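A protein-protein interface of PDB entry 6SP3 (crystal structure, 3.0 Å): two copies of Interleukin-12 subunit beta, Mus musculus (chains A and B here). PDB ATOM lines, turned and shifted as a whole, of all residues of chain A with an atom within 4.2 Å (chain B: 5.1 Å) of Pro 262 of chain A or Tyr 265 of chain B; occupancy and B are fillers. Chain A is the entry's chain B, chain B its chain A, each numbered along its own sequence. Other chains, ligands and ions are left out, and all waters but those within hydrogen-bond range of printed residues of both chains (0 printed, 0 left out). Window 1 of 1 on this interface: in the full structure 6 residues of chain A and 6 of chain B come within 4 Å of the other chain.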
ATOM      1  N   PRO A 198     -26.507  22.438  11.391  1.00  0.00           N
ATOM      2  CA  PRO A 198     -27.121  22.310  10.062  1.00  0.00           C
ATOM      3  C   PRO A 198     -28.490  21.649  10.027  1.00  0.00           C
ATOM      4  O   PRO A 198     -29.456  22.235   9.522  1.00  0.00           O
ATOM      5  CB  PRO A 198     -26.094  21.445   9.313  1.00  0.00           C
ATOM      6  CG  PRO A 198     -24.785  21.851   9.901  1.00  0.00           C
ATOM      7  CD  PRO A 198     -25.054  22.182  11.353  1.00  0.00           C
ATOM      8  N   THR A 199     -28.592  20.448  10.593  1.00  0.00           N
ATOM      9  CA  THR A 199     -29.833  19.685  10.540  1.00  0.00           C
ATOM     10  C   THR A 199     -30.901  20.223  11.483  1.00  0.00           C
ATOM     11  O   THR A 199     -32.086  19.936  11.283  1.00  0.00           O
ATOM     12  CB  THR A 199     -29.544  18.211  10.851  1.00  0.00           C
ATOM     13  OG1 THR A 199     -29.005  17.580   9.681  1.00  0.00           O
ATOM     14  CG2 THR A 199     -30.807  17.469  11.274  1.00  0.00           C
ATOM     15  N   THR A 261     -24.655  22.552   1.705  1.00  0.00           N
ATOM     16  CA  THR A 261     -24.153  21.211   1.465  1.00  0.00           C
ATOM     17  C   THR A 261     -24.313  20.365   2.723  1.00  0.00           C
ATOM     18  O   THR A 261     -24.305  20.902   3.834  1.00  0.00           O
ATOM     19  CB  THR A 261     -22.673  21.245   1.067  1.00  0.00           C
ATOM     20  OG1 THR A 261     -21.901  21.783   2.147  1.00  0.00           O
ATOM     21  CG2 THR A 261     -22.473  22.107  -0.166  1.00  0.00           C
ATOM     22  N   PRO A 262     -24.458  19.035   2.589  1.00  0.00           N
ATOM     23  CA  PRO A 262     -24.508  18.257   1.347  1.00  0.00           C
ATOM     24  C   PRO A 262     -25.854  18.356   0.633  1.00  0.00           C
ATOM     25  O   PRO A 262     -26.894  18.520   1.271  1.00  0.00           O
ATOM     26  CB  PRO A 262     -24.254  16.828   1.827  1.00  0.00           C
ATOM     27  CG  PRO A 262     -24.863  16.801   3.176  1.00  0.00           C
ATOM     28  CD  PRO A 262     -24.608  18.166   3.772  1.00  0.00           C
ATOM     29  N   HIS A 263     -25.819  18.234  -0.693  1.00  0.00           N
ATOM     30  CA  HIS A 263     -27.021  18.396  -1.500  1.00  0.00           C
ATOM     31  C   HIS A 263     -27.990  17.238  -1.321  1.00  0.00           C
ATOM     32  O   HIS A 263     -29.177  17.386  -1.629  1.00  0.00           O
ATOM     33  CB  HIS A 263     -26.625  18.537  -2.968  1.00  0.00           C
ATOM     34  CG  HIS A 263     -25.798  19.752  -3.250  1.00  0.00           C
ATOM     35  ND1 HIS A 263     -26.070  20.620  -4.284  1.00  0.00           N
ATOM     36  CD2 HIS A 263     -24.718  20.257  -2.611  1.00  0.00           C
ATOM     37  CE1 HIS A 263     -25.184  21.601  -4.279  1.00  0.00           C
ATOM     38  NE2 HIS A 263     -24.353  21.406  -3.273  1.00  0.00           N
ATOM     39  N   SER A 264     -27.512  16.092  -0.830  1.00  0.00           N
ATOM     40  CA  SER A 264     -28.413  14.987  -0.529  1.00  0.00           C
ATOM     41  C   SER A 264     -29.394  15.359   0.574  1.00  0.00           C
ATOM     42  O   SER A 264     -30.533  14.879   0.581  1.00  0.00           O
ATOM     43  CB  SER A 264     -27.606  13.753  -0.130  1.00  0.00           C
ATOM     44  OG  SER A 264     -26.491  14.121   0.664  1.00  0.00           O
ATOM     45  N   TYR A 265     -28.972  16.208   1.513  1.00  0.00           N
ATOM     46  CA  TYR A 265     -29.868  16.682   2.558  1.00  0.00           C
ATOM     47  C   TYR A 265     -30.596  17.953   2.139  1.00  0.00           C
ATOM     48  O   TYR A 265     -31.824  18.035   2.241  1.00  0.00           O
ATOM     49  CB  TYR A 265     -29.101  16.939   3.855  1.00  0.00           C
ATOM     50  CG  TYR A 265     -30.019  17.224   5.018  1.00  0.00           C
ATOM     51  CD1 TYR A 265     -30.610  16.188   5.726  1.00  0.00           C
ATOM     52  CD2 TYR A 265     -30.320  18.530   5.391  1.00  0.00           C
ATOM     53  CE1 TYR A 265     -31.459  16.439   6.784  1.00  0.00           C
ATOM     54  CE2 TYR A 265     -31.168  18.792   6.449  1.00  0.00           C
ATOM     55  CZ  TYR A 265     -31.736  17.741   7.140  1.00  0.00           C
ATOM     56  OH  TYR A 265     -32.583  17.990   8.194  1.00  0.00           O
ATOM     57  N   PHE A 266     -29.848  18.952   1.672  1.00  0.00           N
ATOM     58  CA  PHE A 266     -30.424  20.232   1.262  1.00  0.00           C
ATOM     59  C   PHE A 266     -30.832  20.149  -0.209  1.00  0.00           C
ATOM     60  O   PHE A 266     -30.233  20.753  -1.100  1.00  0.00           O
ATOM     61  CB  PHE A 266     -29.435  21.363   1.509  1.00  0.00           C
ATOM     62  CG  PHE A 266     -29.096  21.572   2.957  1.00  0.00           C
ATOM     63  CD1 PHE A 266     -29.995  22.184   3.814  1.00  0.00           C
ATOM     64  CD2 PHE A 266     -27.872  21.162   3.460  1.00  0.00           C
ATOM     65  CE1 PHE A 266     -29.682  22.381   5.147  1.00  0.00           C
ATOM     66  CE2 PHE A 266     -27.552  21.355   4.791  1.00  0.00           C
ATOM     67  CZ  PHE A 266     -28.458  21.965   5.636  1.00  0.00           C
ATOM     68  N   THR B 199     -23.612  17.347  13.387  1.00  0.00           N
ATOM     69  CA  THR B 199     -23.572  17.973  12.070  1.00  0.00           C
ATOM     70  C   THR B 199     -22.648  19.185  12.023  1.00  0.00           C
ATOM     71  O   THR B 199     -22.181  19.549  10.939  1.00  0.00           O
ATOM     72  CB  THR B 199     -24.983  18.399  11.666  1.00  0.00           C
ATOM     73  OG1 THR B 199     -25.602  19.086  12.760  1.00  0.00           O
ATOM     74  CG2 THR B 199     -25.831  17.188  11.317  1.00  0.00           C
ATOM     75  N   PRO B 262     -29.226  11.514  10.167  1.00  0.00           N
ATOM     76  CA  PRO B 262     -29.806  10.857   8.990  1.00  0.00           C
ATOM     77  C   PRO B 262     -28.797  10.598   7.878  1.00  0.00           C
ATOM     78  O   PRO B 262     -27.830  11.343   7.722  1.00  0.00           O
ATOM     79  CB  PRO B 262     -30.869  11.857   8.534  1.00  0.00           C
ATOM     80  CG  PRO B 262     -30.291  13.174   8.896  1.00  0.00           C
ATOM     81  CD  PRO B 262     -29.556  12.952  10.198  1.00  0.00           C
ATOM     82  N   HIS B 263     -29.045   9.540   7.105  1.00  0.00           N
ATOM     83  CA  HIS B 263     -28.112   9.126   6.064  1.00  0.00           C
ATOM     84  C   HIS B 263     -28.092  10.091   4.889  1.00  0.00           C
ATOM     85  O   HIS B 263     -27.134  10.079   4.110  1.00  0.00           O
ATOM     86  CB  HIS B 263     -28.478   7.721   5.599  1.00  0.00           C
ATOM     87  CG  HIS B 263     -28.336   6.679   6.666  1.00  0.00           C
ATOM     88  ND1 HIS B 263     -27.703   5.474   6.453  1.00  0.00           N
ATOM     89  CD2 HIS B 263     -28.724   6.676   7.963  1.00  0.00           C
ATOM     90  CE1 HIS B 263     -27.725   4.765   7.568  1.00  0.00           C
ATOM     91  NE2 HIS B 263     -28.336   5.473   8.501  1.00  0.00           N
ATOM     92  N   SER B 264     -29.133  10.913   4.737  1.00  0.00           N
ATOM     93  CA  SER B 264     -29.116  11.947   3.708  1.00  0.00           C
ATOM     94  C   SER B 264     -28.036  12.987   3.980  1.00  0.00           C
ATOM     95  O   SER B 264     -27.470  13.553   3.038  1.00  0.00           O
ATOM     96  CB  SER B 264     -30.491  12.603   3.616  1.00  0.00           C
ATOM     97  OG  SER B 264     -31.052  12.769   4.906  1.00  0.00           O
ATOM     98  N   TYR B 265     -27.734  13.249   5.253  1.00  0.00           N
ATOM     99  CA  TYR B 265     -26.665  14.174   5.611  1.00  0.00           C
ATOM    100  C   TYR B 265     -25.319  13.469   5.726  1.00  0.00           C
ATOM    101  O   TYR B 265     -24.330  13.909   5.132  1.00  0.00           O
ATOM    102  CB  TYR B 265     -26.978  14.873   6.936  1.00  0.00           C
ATOM    103  CG  TYR B 265     -26.014  15.994   7.255  1.00  0.00           C
ATOM    104  CD1 TYR B 265     -26.191  17.265   6.724  1.00  0.00           C
ATOM    105  CD2 TYR B 265     -24.905  15.770   8.062  1.00  0.00           C
ATOM    106  CE1 TYR B 265     -25.305  18.287   7.010  1.00  0.00           C
ATOM    107  CE2 TYR B 265     -24.012  16.783   8.348  1.00  0.00           C
ATOM    108  CZ  TYR B 265     -24.215  18.038   7.818  1.00  0.00           C
ATOM    109  OH  TYR B 265     -23.326  19.050   8.102  1.00  0.00           O
ATOM    110  N   PHE B 266     -25.268  12.385   6.500  1.00  0.00           N
ATOM    111  CA  PHE B 266     -24.033  11.629   6.706  1.00  0.00           C
ATOM    112  C   PHE B 266     -23.914  10.570   5.610  1.00  0.00           C
ATOM    113  O   PHE B 266     -24.021   9.364   5.839  1.00  0.00           O
ATOM    114  CB  PHE B 266     -24.018  11.006   8.096  1.00  0.00           C
ATOM    115  CG  PHE B 266     -24.015  12.012   9.214  1.00  0.00           C
ATOM    116  CD1 PHE B 266     -22.866  12.718   9.526  1.00  0.00           C
ATOM    117  CD2 PHE B 266     -25.163  12.245   9.956  1.00  0.00           C
ATOM    118  CE1 PHE B 266     -22.860  13.642  10.557  1.00  0.00           C
ATOM    119  CE2 PHE B 266     -25.164  13.165  10.988  1.00  0.00           C
ATOM    120  CZ  PHE B 266     -24.011  13.864  11.289  1.00  0.00           C
ATOM    121  N   SER B 267     -23.683  11.054   4.392  1.00  0.00           N
ATOM    122  CA  SER B 267     -23.620  10.163   3.244  1.00  0.00           C
ATOM    123  C   SER B 267     -22.327   9.355   3.253  1.00  0.00           C
ATOM    124  O   SER B 267     -21.336   9.710   3.899  1.00  0.00           O
ATOM    125  CB  SER B 267     -23.729  10.952   1.941  1.00  0.00           C
ATOM    126  OG  SER B 267     -24.957  11.650   1.867  1.00  0.00           O
ATOM    127  N   TYR B 318     -17.573  12.566   1.818  1.00  0.00           N
ATOM    128  CA  TYR B 318     -17.042  13.907   1.609  1.00  0.00           C
ATOM    129  C   TYR B 318     -15.654  14.144   2.192  1.00  0.00           C
ATOM    130  O   TYR B 318     -14.964  15.058   1.729  1.00  0.00           O
ATOM    131  CB  TYR B 318     -18.023  14.935   2.184  1.00  0.00           C
ATOM    132  CG  TYR B 318     -19.440  14.685   1.724  1.00  0.00           C
ATOM    133  CD1 TYR B 318     -19.773  14.780   0.380  1.00  0.00           C
ATOM    134  CD2 TYR B 318     -20.434  14.326   2.622  1.00  0.00           C
ATOM    135  CE1 TYR B 318     -21.057  14.545  -0.054  1.00  0.00           C
ATOM    136  CE2 TYR B 318     -21.723  14.085   2.196  1.00  0.00           C
ATOM    137  CZ  TYR B 318     -22.027  14.195   0.856  1.00  0.00           C
ATOM    138  OH  TYR B 318     -23.312  13.958   0.423  1.00  0.00           O
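Printed residues of chain B that touch a printed residue of chain A: Thr 199, Ser 264, Tyr 265, Ser 267 and Tyr 318. Hydrophobic or aromatic side chains of chain B within 4 Å of the printed part of chain A: Tyr 265 and Tyr 318. Printed residues of chain A that touch a printed residue of chain B: Pro 198, Thr 199, Pro 262, Ser 264 and Tyr 265. Along chain A the printed residues that touch a printed residue of chain B span positions 198 to 265. Among the printed residues, no Asp or Glu carboxylate lies within 4 Å of a Lys or Arg side-chain nitrogen of the other chain.
The backbone carbonyl oxygen (O) of Thr 199 of chain B lies within hydrogen-bond range of the side-chain hydroxyl (OH) of Tyr 265 of chain B, at 3.1 Å. The backbone carbonyl oxygen (O) of His 263 of chain B sits at hydrogen-bond distance from the side-chain hydroxyl (OG) of Ser 267 of chain B (3.5 Å). O of Ser 264 of chain B sits at hydrogen-bond distance from OG of Ser 267 of chain B (3.4 Å). The side-chain hydroxyl of Tyr 318 of chain B lies within hydrogen-bond range of the side-chain hydroxyl of Ser 267 of chain B, 3.2 Å away.
The backbone carbonyl oxygen of Ser 264 of chain B sits at hydrogen-bond distance from the side-chain hydroxyl of Ser 264 of chain A, at 2.6 Å. The backbone NH (N) of Tyr 265 of chain A is in hydrogen-bond range of the backbone carbonyl oxygen (O) of Ser 264 of chain B, at 3.4 Å. OG of Ser 264 of chain A is in hydrogen-bond range of OG of Ser 267 of chain B, at 3.1 Å. OH of Tyr 318 of chain B lies within hydrogen-bond range of OG of Ser 264 of chain A (3.2 Å).
Thr 199 of chain B touches its own counterpart, Thr 199 of chain A. Pro 262 of chain A touches Tyr 265 of chain B, but with the chains exchanged Tyr 265 of chain A does not touch Pro 262 of chain B (4.1 Å). Ser 264 of chain A touches its own counterpart, Ser 264 of chain B. Tyr 265 of chain A touches Ser 264 of chain B, but with the chains exchanged Ser 264 of chain A does not touch Tyr 265 of chain B (4.8 Å). 6 positions are printed for both chains. Of the 9 pairs that touch across the chains among the printed residues, 2 have their exchanged pair printed and touching as well.
Pro 198 of chain A touches Thr 199 of chain B (CD to OG1, 3.4 Å). Pro 198 of chain A touches Tyr 265 of chain B. OG1 of Thr 199 of chain A touches CG2 of Thr 199 of chain B, 3.6 Å away. Pro 262 of chain A touches Tyr 265 of chain B. Pro 262 of chain A touches Tyr 318 of chain B.
Pro 262 of chain A touches two residues of chain B. Tyr 265 of chain B touches just these residues of chain A: Pro 198 (3.6 Å) and Pro 262 (3.3 Å). Of the printed residues of chain B, Thr 199 of chain A touches Thr 199 (3.6 Å). Of the printed residues of chain A, Ser 267 of chain B touches Ser 264 (3.1 Å). Of the printed residues of chain A, Tyr 318 of chain B touches Pro 262 and Ser 264.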
